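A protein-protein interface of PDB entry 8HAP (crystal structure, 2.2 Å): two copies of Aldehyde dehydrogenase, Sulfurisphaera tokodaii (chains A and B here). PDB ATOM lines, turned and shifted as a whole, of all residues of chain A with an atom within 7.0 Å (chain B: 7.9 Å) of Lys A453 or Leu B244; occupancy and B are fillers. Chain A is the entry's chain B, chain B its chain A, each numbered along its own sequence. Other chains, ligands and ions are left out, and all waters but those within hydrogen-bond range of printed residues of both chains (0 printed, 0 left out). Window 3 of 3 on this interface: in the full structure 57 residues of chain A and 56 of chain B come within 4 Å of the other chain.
O of Gly B223 is in hydrogen-bond range of N of Arg B247, at 3.2 Å.
N of Ile B225 lies within hydrogen-bond range of O of Arg B247, at 3.0 Å.
OG of Ser B243 sits at hydrogen-bond distance from O of Lys B240, 2.4 Å away.
O of Glu A406 lies within hydrogen-bond range of N of Lys A453.
NZ of Lys A452 lies within hydrogen-bond range of O of Tyr A407.
The backbone NH (N) of Phe A451 is in hydrogen-bond range of the backbone carbonyl oxygen (O) of Gly A408 (3.1 Å).
The side-chain hydroxyl (OG) of Ser B239 lies within hydrogen-bond range of the backbone carbonyl oxygen (O) of Ser A239 (2.8 Å).
The backbone carbonyl oxygen of Gly A450 sits at hydrogen-bond distance from the guanidinium group of Arg B247 (3.0 Å).
NH1 of Arg B247 is in hydrogen-bond range of O of Lys A452.
NH2 of Arg B247 lies within hydrogen-bond range of O of Gly A455 (3.1 Å).
Ser A239 touches its own counterpart, Ser B239.
Of the 11 pairs that touch across the chains among the printed residues, 1 has its exchanged pair printed and touching as well.
Of the 18 printed residues of chain B, 6 touch a printed residue of chain A.
Printed residues of chain B that touch a printed residue of chain A: Ser B239, Val B242, Ser B243, Leu B244, Gly B245 and Arg B247.
Hydrophobic or aromatic side chains of chain B that line the printed part of chain A: Val B242.
Of the 18 printed residues of chain A, 7 touch a printed residue of chain B.
Hydrophobic or aromatic side chains of chain A that line the printed part of chain B: Leu A235.
Among the printed residues, 11 pairs touch across the chains.
Among the printed residues, no Asp or Glu carboxylate lies within 4 Å of a Lys or Arg side-chain nitrogen of the other chain.
Among the printed residues, pairs that only touch across the chains: Leu A235 with Val B242 (3.6 Å), Phe A451 with Arg B247 (3.6 Å), Ser A239 with Ser B243 (3.7 Å), Ser A239 with Val B242 (3.7 Å), Lys A453 with Leu B244 (3.7 Å), Leu A235 with Ser B243 (3.8 Å) and Leu A235 with Gly B245 (3.9 Å).
Lys A453 touches just one residue of chain B: Leu B244 (3.7 Å).
Of chain A, only Lys A453 comes within 4 Å of Leu B244.
Printed residues of chain A within 4 Å of Val B242: Leu A235 and Ser A239.
Printed residues of chain B within 4 Å of Gly A455: Arg B247 (3.1 Å).
Of the printed residues of chain B, Leu A235 touches Val B242, Ser B243 and Gly B245.
Of the printed residues of chain A, Ser B243 touches Leu A235 (3.8 Å) and Ser A239 (3.7 Å).
Printed residues of chain A within 4 Å of Ser B239: Ser A239.
The nearest residue of chain B that does not touch Lys A453 is Gly B245 (4.5 Å).
The nearest residue of chain A that does not touch Leu B244 is Leu A235 (4.3 Å).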
ATOM      1  N   SER A 230      16.496  11.128  -6.198  1.00  0.00           N
ATOM      2  CA  SER A 230      15.683  10.937  -4.972  1.00  0.00           C
ATOM      3  C   SER A 230      14.561   9.940  -5.274  1.00  0.00           C
ATOM      4  O   SER A 230      14.210   9.796  -6.458  1.00  0.00           O
ATOM      5  CB  SER A 230      15.183  12.268  -4.452  1.00  0.00           C
ATOM      6  OG  SER A 230      14.042  12.714  -5.157  1.00  0.00           O
ATOM      7  N   THR A 231      14.106   9.202  -4.260  1.00  0.00           N
ATOM      8  CA  THR A 231      12.970   8.252  -4.334  1.00  0.00           C
ATOM      9  C   THR A 231      11.716   8.923  -4.921  1.00  0.00           C
ATOM     10  O   THR A 231      11.136   8.328  -5.836  1.00  0.00           O
ATOM     11  CB  THR A 231      12.677   7.630  -2.963  1.00  0.00           C
ATOM     12  OG1 THR A 231      13.709   6.676  -2.710  1.00  0.00           O
ATOM     13  CG2 THR A 231      11.344   6.922  -2.915  1.00  0.00           C
ATOM     14  N   LEU A 235      10.386   7.667  -8.735  1.00  0.00           N
ATOM     15  CA  LEU A 235       9.182   6.799  -8.803  1.00  0.00           C
ATOM     16  C   LEU A 235       8.105   7.466  -9.675  1.00  0.00           C
ATOM     17  O   LEU A 235       7.482   6.753 -10.492  1.00  0.00           O
ATOM     18  CB  LEU A 235       8.703   6.481  -7.381  1.00  0.00           C
ATOM     19  CG  LEU A 235       9.636   5.582  -6.560  1.00  0.00           C
ATOM     20  CD1 LEU A 235       8.972   5.119  -5.272  1.00  0.00           C
ATOM     21  CD2 LEU A 235      10.113   4.382  -7.355  1.00  0.00           C
ATOM     22  N   SER A 239       7.031   5.730 -13.130  1.00  0.00           N
ATOM     23  CA  SER A 239       5.569   5.582 -13.302  1.00  0.00           C
ATOM     24  C   SER A 239       5.148   6.079 -14.690  1.00  0.00           C
ATOM     25  O   SER A 239       4.558   5.286 -15.454  1.00  0.00           O
ATOM     26  CB  SER A 239       4.833   6.294 -12.200  1.00  0.00           C
ATOM     27  OG  SER A 239       3.441   6.091 -12.342  1.00  0.00           O
ATOM     28  N   GLU A 251      18.304   4.182  -9.707  1.00  0.00           N
ATOM     29  CA  GLU A 251      19.142   4.094  -8.482  1.00  0.00           C
ATOM     30  C   GLU A 251      18.740   5.287  -7.609  1.00  0.00           C
ATOM     31  O   GLU A 251      19.037   6.446  -7.936  1.00  0.00           O
ATOM     32  CB  GLU A 251      20.628   3.979  -8.829  1.00  0.00           C
ATOM     33  CG  GLU A 251      20.927   2.913  -9.885  1.00  0.00           C
ATOM     34  CD  GLU A 251      20.798   1.461  -9.417  1.00  0.00           C
ATOM     35  OE1 GLU A 251      21.639   1.061  -8.606  1.00  0.00           O
ATOM     36  OE2 GLU A 251      19.861   0.717  -9.869  1.00  0.00           O
ATOM     37  N   LEU A 252      17.928   5.018  -6.603  1.00  0.00           N
ATOM     38  CA  LEU A 252      17.294   6.077  -5.793  1.00  0.00           C
ATOM     39  C   LEU A 252      18.037   6.098  -4.443  1.00  0.00           C
ATOM     40  O   LEU A 252      19.208   5.663  -4.396  1.00  0.00           O
ATOM     41  CB  LEU A 252      15.786   5.783  -5.753  1.00  0.00           C
ATOM     42  CG  LEU A 252      15.131   5.594  -7.136  1.00  0.00           C
ATOM     43  CD1 LEU A 252      13.610   5.465  -7.051  1.00  0.00           C
ATOM     44  CD2 LEU A 252      15.497   6.723  -8.082  1.00  0.00           C
ATOM     45  N   GLY A 253      17.446   6.592  -3.379  1.00  0.00           N
ATOM     46  CA  GLY A 253      18.226   6.822  -2.140  1.00  0.00           C
ATOM     47  C   GLY A 253      18.693   5.558  -1.405  1.00  0.00           C
ATOM     48  O   GLY A 253      18.396   4.397  -1.805  1.00  0.00           O
ATOM     49  N   GLY A 254      19.443   5.790  -0.334  1.00  0.00           N
ATOM     50  CA  GLY A 254      19.593   4.830   0.764  1.00  0.00           C
ATOM     51  C   GLY A 254      19.721   5.549   2.079  1.00  0.00           C
ATOM     52  O   GLY A 254      19.921   6.777   2.068  1.00  0.00           O
ATOM     53  N   GLU A 406      12.559   2.426   4.571  1.00  0.00           N
ATOM     54  CA  GLU A 406      11.963   2.107   3.245  1.00  0.00           C
ATOM     55  C   GLU A 406      13.078   1.826   2.222  1.00  0.00           C
ATOM     56  O   GLU A 406      12.732   1.506   1.062  1.00  0.00           O
ATOM     57  CB  GLU A 406      11.088   3.274   2.762  1.00  0.00           C
ATOM     58  CG  GLU A 406      11.845   4.594   2.620  1.00  0.00           C
ATOM     59  CD  GLU A 406      11.102   5.692   1.883  1.00  0.00           C
ATOM     60  OE1 GLU A 406      11.759   6.513   1.215  1.00  0.00           O
ATOM     61  OE2 GLU A 406       9.870   5.719   1.982  1.00  0.00           O
ATOM     62  N   TYR A 407      14.354   1.986   2.617  1.00  0.00           N
ATOM     63  CA  TYR A 407      15.554   1.843   1.746  1.00  0.00           C
ATOM     64  C   TYR A 407      16.174   0.451   1.928  1.00  0.00           C
ATOM     65  O   TYR A 407      15.818  -0.253   2.900  1.00  0.00           O
ATOM     66  CB  TYR A 407      16.536   2.985   2.034  1.00  0.00           C
ATOM     67  CG  TYR A 407      15.995   4.361   1.726  1.00  0.00           C
ATOM     68  CD1 TYR A 407      15.736   4.729   0.417  1.00  0.00           C
ATOM     69  CD2 TYR A 407      15.723   5.291   2.716  1.00  0.00           C
ATOM     70  CE1 TYR A 407      15.238   5.980   0.096  1.00  0.00           C
ATOM     71  CE2 TYR A 407      15.220   6.547   2.412  1.00  0.00           C
ATOM     72  CZ  TYR A 407      14.969   6.889   1.096  1.00  0.00           C
ATOM     73  OH  TYR A 407      14.476   8.108   0.732  1.00  0.00           O
ATOM     74  N   GLY A 408      17.083   0.049   1.028  1.00  0.00           N
ATOM     75  CA  GLY A 408      17.776  -1.255   1.124  1.00  0.00           C
ATOM     76  C   GLY A 408      19.028  -1.324   0.262  1.00  0.00           C
ATOM     77  O   GLY A 408      19.231  -2.338  -0.429  1.00  0.00           O
ATOM     78  N   GLY A 450      19.580  -2.077  -4.665  1.00  0.00           N
ATOM     79  CA  GLY A 450      19.008  -2.895  -3.585  1.00  0.00           C
ATOM     80  C   GLY A 450      17.491  -2.998  -3.583  1.00  0.00           C
ATOM     81  O   GLY A 450      16.859  -2.892  -4.641  1.00  0.00           O
ATOM     82  N   PHE A 451      16.947  -3.241  -2.393  1.00  0.00           N
ATOM     83  CA  PHE A 451      15.564  -3.707  -2.138  1.00  0.00           C
ATOM     84  C   PHE A 451      14.643  -2.497  -2.006  1.00  0.00           C
ATOM     85  O   PHE A 451      15.132  -1.322  -1.940  1.00  0.00           O
ATOM     86  CB  PHE A 451      15.518  -4.525  -0.847  1.00  0.00           C
ATOM     87  CG  PHE A 451      16.169  -5.884  -0.906  1.00  0.00           C
ATOM     88  CD1 PHE A 451      17.488  -6.041  -1.311  1.00  0.00           C
ATOM     89  CD2 PHE A 451      15.458  -7.015  -0.523  1.00  0.00           C
ATOM     90  CE1 PHE A 451      18.077  -7.301  -1.341  1.00  0.00           C
ATOM     91  CE2 PHE A 451      16.047  -8.271  -0.550  1.00  0.00           C
ATOM     92  CZ  PHE A 451      17.360  -8.409  -0.949  1.00  0.00           C
ATOM     93  N   LYS A 452      13.340  -2.773  -1.930  1.00  0.00           N
ATOM     94  CA  LYS A 452      12.330  -1.771  -1.518  1.00  0.00           C
ATOM     95  C   LYS A 452      12.541  -0.567  -2.442  1.00  0.00           C
ATOM     96  O   LYS A 452      12.806  -0.815  -3.638  1.00  0.00           O
ATOM     97  CB  LYS A 452      12.488  -1.497  -0.012  1.00  0.00           C
ATOM     98  CG  LYS A 452      12.164  -2.674   0.902  1.00  0.00           C
ATOM     99  CD  LYS A 452      13.112  -2.833   2.071  1.00  0.00           C
ATOM    100  CE  LYS A 452      12.728  -2.010   3.284  1.00  0.00           C
ATOM    101  NZ  LYS A 452      13.626  -2.268   4.434  1.00  0.00           N
ATOM    102  N   LYS A 453      12.515   0.662  -1.918  1.00  0.00           N
ATOM    103  CA  LYS A 453      12.435   1.917  -2.720  1.00  0.00           C
ATOM    104  C   LYS A 453      13.832   2.476  -2.993  1.00  0.00           C
ATOM    105  O   LYS A 453      13.940   3.661  -3.355  1.00  0.00           O
ATOM    106  CB  LYS A 453      11.543   2.930  -1.996  1.00  0.00           C
ATOM    107  CG  LYS A 453      10.087   2.491  -1.927  1.00  0.00           C
ATOM    108  CD  LYS A 453       9.137   3.613  -1.640  1.00  0.00           C
ATOM    109  CE  LYS A 453       7.811   3.104  -1.127  1.00  0.00           C
ATOM    110  NZ  LYS A 453       6.897   4.234  -0.866  1.00  0.00           N
ATOM    111  N   THR A 454      14.861   1.642  -2.858  1.00  0.00           N
ATOM    112  CA  THR A 454      16.262   1.997  -3.199  1.00  0.00           C
ATOM    113  C   THR A 454      16.411   2.056  -4.729  1.00  0.00           C
ATOM    114  O   THR A 454      17.304   2.777  -5.200  1.00  0.00           O
ATOM    115  CB  THR A 454      17.245   1.064  -2.490  1.00  0.00           C
ATOM    116  OG1 THR A 454      17.526   1.734  -1.256  1.00  0.00           O
ATOM    117  CG2 THR A 454      18.502   0.794  -3.293  1.00  0.00           C
ATOM    118  N   GLY A 455      15.551   1.361  -5.473  1.00  0.00           N
ATOM    119  CA  GLY A 455      15.450   1.551  -6.932  1.00  0.00           C
ATOM    120  C   GLY A 455      14.783   0.396  -7.650  1.00  0.00           C
ATOM    121  O   GLY A 455      14.107  -0.419  -6.990  1.00  0.00           O
ATOM    122  N   ILE A 456      14.962   0.369  -8.970  1.00  0.00           N
ATOM    123  CA  ILE A 456      14.581  -0.745  -9.884  1.00  0.00           C
ATOM    124  C   ILE A 456      15.818  -1.165 -10.675  1.00  0.00           C
ATOM    125  O   ILE A 456      16.404  -0.335 -11.402  1.00  0.00           O
ATOM    126  CB  ILE A 456      13.405  -0.382 -10.806  1.00  0.00           C
ATOM    127  CG1 ILE A 456      12.198   0.095  -9.994  1.00  0.00           C
ATOM    128  CG2 ILE A 456      13.032  -1.570 -11.700  1.00  0.00           C
ATOM    129  CD1 ILE A 456      12.003   1.590 -10.007  1.00  0.00           C
ATOM    130  N   ASP B 214      -7.268  -3.186  -7.367  1.00  0.00           N
ATOM    131  CA  ASP B 214      -6.382  -2.108  -6.847  1.00  0.00           C
ATOM    132  C   ASP B 214      -5.587  -2.576  -5.616  1.00  0.00           C
ATOM    133  O   ASP B 214      -4.372  -2.379  -5.607  1.00  0.00           O
ATOM    134  CB  ASP B 214      -7.180  -0.842  -6.559  1.00  0.00           C
ATOM    135  CG  ASP B 214      -6.461   0.365  -7.102  1.00  0.00           C
ATOM    136  OD1 ASP B 214      -6.220   0.375  -8.325  1.00  0.00           O
ATOM    137  OD2 ASP B 214      -6.085   1.242  -6.294  1.00  0.00           O
ATOM    138  N   ILE B 217      -2.437  -4.500  -6.228  1.00  0.00           N
ATOM    139  CA  ILE B 217      -1.363  -3.692  -6.869  1.00  0.00           C
ATOM    140  C   ILE B 217      -0.750  -2.720  -5.854  1.00  0.00           C
ATOM    141  O   ILE B 217       0.433  -2.349  -6.053  1.00  0.00           O
ATOM    142  CB  ILE B 217      -1.888  -2.949  -8.123  1.00  0.00           C
ATOM    143  CG1 ILE B 217      -2.527  -3.894  -9.144  1.00  0.00           C
ATOM    144  CG2 ILE B 217      -0.777  -2.140  -8.762  1.00  0.00           C
ATOM    145  CD1 ILE B 217      -1.714  -5.157  -9.425  1.00  0.00           C
ATOM    146  N   THR B 218      -1.517  -2.271  -4.855  1.00  0.00           N
ATOM    147  CA  THR B 218      -1.156  -1.120  -3.980  1.00  0.00           C
ATOM    148  C   THR B 218      -0.774  -1.584  -2.561  1.00  0.00           C
ATOM    149  O   THR B 218      -0.074  -0.841  -1.880  1.00  0.00           O
ATOM    150  CB  THR B 218      -2.300  -0.098  -3.928  1.00  0.00           C
ATOM    151  OG1 THR B 218      -3.457  -0.826  -3.527  1.00  0.00           O
ATOM    152  CG2 THR B 218      -2.569   0.572  -5.253  1.00  0.00           C
ATOM    153  N   HIS B 219      -1.215  -2.750  -2.096  1.00  0.00           N
ATOM    154  CA  HIS B 219      -0.937  -3.165  -0.697  1.00  0.00           C
ATOM    155  C   HIS B 219       0.558  -3.053  -0.424  1.00  0.00           C
ATOM    156  O   HIS B 219       1.352  -3.454  -1.267  1.00  0.00           O
ATOM    157  CB  HIS B 219      -1.423  -4.578  -0.430  1.00  0.00           C
ATOM    158  CG  HIS B 219      -1.628  -4.807   1.020  1.00  0.00           C
ATOM    159  ND1 HIS B 219      -0.587  -4.880   1.890  1.00  0.00           N
ATOM    160  CD2 HIS B 219      -2.754  -4.937   1.752  1.00  0.00           C
ATOM    161  CE1 HIS B 219      -1.045  -5.040   3.110  1.00  0.00           C
ATOM    162  NE2 HIS B 219      -2.372  -5.098   3.050  1.00  0.00           N
ATOM    163  N   PRO B 220       0.993  -2.470   0.720  1.00  0.00           N
ATOM    164  CA  PRO B 220       2.420  -2.309   1.004  1.00  0.00           C
ATOM    165  C   PRO B 220       3.163  -3.646   1.111  1.00  0.00           C
ATOM    166  O   PRO B 220       4.354  -3.634   1.040  1.00  0.00           O
ATOM    167  CB  PRO B 220       2.487  -1.598   2.367  1.00  0.00           C
ATOM    168  CG  PRO B 220       1.114  -0.947   2.521  1.00  0.00           C
ATOM    169  CD  PRO B 220       0.148  -1.832   1.747  1.00  0.00           C
ATOM    170  N   VAL B 222       2.973  -6.182  -0.942  1.00  0.00           N
ATOM    171  CA  VAL B 222       3.176  -6.760  -2.309  1.00  0.00           C
ATOM    172  C   VAL B 222       4.538  -6.248  -2.796  1.00  0.00           C
ATOM    173  O   VAL B 222       4.724  -5.045  -2.853  1.00  0.00           O
ATOM    174  CB  VAL B 222       2.014  -6.408  -3.260  1.00  0.00           C
ATOM    175  CG1 VAL B 222       2.241  -6.810  -4.717  1.00  0.00           C
ATOM    176  CG2 VAL B 222       0.699  -6.987  -2.763  1.00  0.00           C
ATOM    177  N   GLY B 223       5.471  -7.143  -3.101  1.00  0.00           N
ATOM    178  CA  GLY B 223       6.824  -6.778  -3.576  1.00  0.00           C
ATOM    179  C   GLY B 223       6.900  -6.705  -5.087  1.00  0.00           C
ATOM    180  O   GLY B 223       7.812  -6.014  -5.612  1.00  0.00           O
ATOM    181  N   ILE B 225       4.577  -7.604  -9.071  1.00  0.00           N
ATOM    182  CA  ILE B 225       3.360  -7.898  -9.847  1.00  0.00           C
ATOM    183  C   ILE B 225       3.778  -8.522 -11.169  1.00  0.00           C
ATOM    184  O   ILE B 225       4.454  -7.858 -11.928  1.00  0.00           O
ATOM    185  CB  ILE B 225       2.520  -6.628 -10.062  1.00  0.00           C
ATOM    186  CG1 ILE B 225       1.893  -6.142  -8.746  1.00  0.00           C
ATOM    187  CG2 ILE B 225       1.486  -6.928 -11.125  1.00  0.00           C
ATOM    188  CD1 ILE B 225       2.445  -4.852  -8.244  1.00  0.00           C
ATOM    189  N   ALA B 238       1.037  -1.568 -14.414  1.00  0.00           N
ATOM    190  CA  ALA B 238       2.513  -1.454 -14.288  1.00  0.00           C
ATOM    191  C   ALA B 238       2.893  -0.074 -13.748  1.00  0.00           C
ATOM    192  O   ALA B 238       3.718   0.010 -12.833  1.00  0.00           O
ATOM    193  CB  ALA B 238       3.165  -1.704 -15.612  1.00  0.00           C
ATOM    194  N   SER B 239       2.282   0.963 -14.310  1.00  0.00           N
ATOM    195  CA  SER B 239       2.459   2.376 -13.918  1.00  0.00           C
ATOM    196  C   SER B 239       2.153   2.545 -12.431  1.00  0.00           C
ATOM    197  O   SER B 239       2.952   3.170 -11.706  1.00  0.00           O
ATOM    198  CB  SER B 239       1.614   3.285 -14.771  1.00  0.00           C
ATOM    199  OG  SER B 239       1.972   4.629 -14.502  1.00  0.00           O
ATOM    200  N   LYS B 240       1.027   2.018 -11.975  1.00  0.00           N
ATOM    201  CA  LYS B 240       0.641   2.068 -10.545  1.00  0.00           C
ATOM    202  C   LYS B 240       1.663   1.274  -9.703  1.00  0.00           C
ATOM    203  O   LYS B 240       2.150   1.789  -8.679  1.00  0.00           O
ATOM    204  CB  LYS B 240      -0.779   1.520 -10.373  1.00  0.00           C
ATOM    205  CG  LYS B 240      -1.367   1.755  -8.989  1.00  0.00           C
ATOM    206  CD  LYS B 240      -2.576   2.684  -8.962  1.00  0.00           C
ATOM    207  CE  LYS B 240      -3.698   2.273  -9.903  1.00  0.00           C
ATOM    208  NZ  LYS B 240      -4.013   0.821  -9.817  1.00  0.00           N
ATOM    209  N   ALA B 241       1.994   0.049 -10.086  1.00  0.00           N
ATOM    210  CA  ALA B 241       2.948  -0.767  -9.298  1.00  0.00           C
ATOM    211  C   ALA B 241       4.248   0.026  -9.115  1.00  0.00           C
ATOM    212  O   ALA B 241       4.720   0.184  -7.961  1.00  0.00           O
ATOM    213  CB  ALA B 241       3.188  -2.096  -9.959  1.00  0.00           C
ATOM    214  N   VAL B 242       4.773   0.567 -10.207  1.00  0.00           N
ATOM    215  CA  VAL B 242       6.130   1.180 -10.239  1.00  0.00           C
ATOM    216  C   VAL B 242       6.152   2.483  -9.425  1.00  0.00           C
ATOM    217  O   VAL B 242       7.197   2.733  -8.787  1.00  0.00           O
ATOM    218  CB  VAL B 242       6.568   1.384 -11.690  1.00  0.00           C
ATOM    219  CG1 VAL B 242       7.727   2.354 -11.790  1.00  0.00           C
ATOM    220  CG2 VAL B 242       6.949   0.045 -12.304  1.00  0.00           C
ATOM    221  N   SER B 243       5.032   3.229  -9.407  1.00  0.00           N
ATOM    222  CA  SER B 243       4.811   4.465  -8.605  1.00  0.00           C
ATOM    223  C   SER B 243       5.015   4.193  -7.110  1.00  0.00           C
ATOM    224  O   SER B 243       5.298   5.151  -6.410  1.00  0.00           O
ATOM    225  CB  SER B 243       3.424   5.055  -8.832  1.00  0.00           C
ATOM    226  OG  SER B 243       2.395   4.195  -8.327  1.00  0.00           O
ATOM    227  N   LEU B 244       4.821   2.954  -6.638  1.00  0.00           N
ATOM    228  CA  LEU B 244       4.972   2.581  -5.206  1.00  0.00           C
ATOM    229  C   LEU B 244       6.248   1.761  -4.995  1.00  0.00           C
ATOM    230  O   LEU B 244       6.358   1.149  -3.922  1.00  0.00           O
ATOM    231  CB  LEU B 244       3.743   1.795  -4.752  1.00  0.00           C
ATOM    232  CG  LEU B 244       2.389   2.460  -5.013  1.00  0.00           C
ATOM    233  CD1 LEU B 244       1.266   1.481  -4.732  1.00  0.00           C
ATOM    234  CD2 LEU B 244       2.204   3.717  -4.171  1.00  0.00           C
ATOM    235  N   GLY B 245       7.162   1.728  -5.969  1.00  0.00           N
ATOM    236  CA  GLY B 245       8.466   1.043  -5.837  1.00  0.00           C
ATOM    237  C   GLY B 245       8.379  -0.464  -6.016  1.00  0.00           C
ATOM    238  O   GLY B 245       9.362  -1.148  -5.658  1.00  0.00           O
ATOM    239  N   LYS B 246       7.275  -0.985  -6.568  1.00  0.00           N
ATOM    240  CA  LYS B 246       7.076  -2.450  -6.742  1.00  0.00           C
ATOM    241  C   LYS B 246       7.691  -2.907  -8.074  1.00  0.00           C
ATOM    242  O   LYS B 246       7.647  -2.121  -9.037  1.00  0.00           O
ATOM    243  CB  LYS B 246       5.584  -2.780  -6.676  1.00  0.00           C
ATOM    244  CG  LYS B 246       4.912  -2.355  -5.382  1.00  0.00           C
ATOM    245  CD  LYS B 246       3.506  -2.855  -5.267  1.00  0.00           C
ATOM    246  CE  LYS B 246       2.767  -2.197  -4.133  1.00  0.00           C
ATOM    247  NZ  LYS B 246       3.350  -2.595  -2.824  1.00  0.00           N
ATOM    248  N   ARG B 247       8.243  -4.129  -8.123  1.00  0.00           N
ATOM    249  CA  ARG B 247       8.813  -4.739  -9.362  1.00  0.00           C
ATOM    250  C   ARG B 247       7.628  -5.241 -10.196  1.00  0.00           C
ATOM    251  O   ARG B 247       6.559  -5.482  -9.605  1.00  0.00           O
ATOM    252  CB  ARG B 247       9.786  -5.899  -9.077  1.00  0.00           C
ATOM    253  CG  ARG B 247      11.191  -5.492  -8.647  1.00  0.00           C
ATOM    254  CD  ARG B 247      11.219  -4.836  -7.277  1.00  0.00           C
ATOM    255  NE  ARG B 247      12.538  -4.400  -6.824  1.00  0.00           N
ATOM    256  CZ  ARG B 247      12.763  -3.444  -5.906  1.00  0.00           C
ATOM    257  NH1 ARG B 247      11.756  -2.781  -5.358  1.00  0.00           N
ATOM    258  NH2 ARG B 247      14.000  -3.152  -5.538  1.00  0.00           N
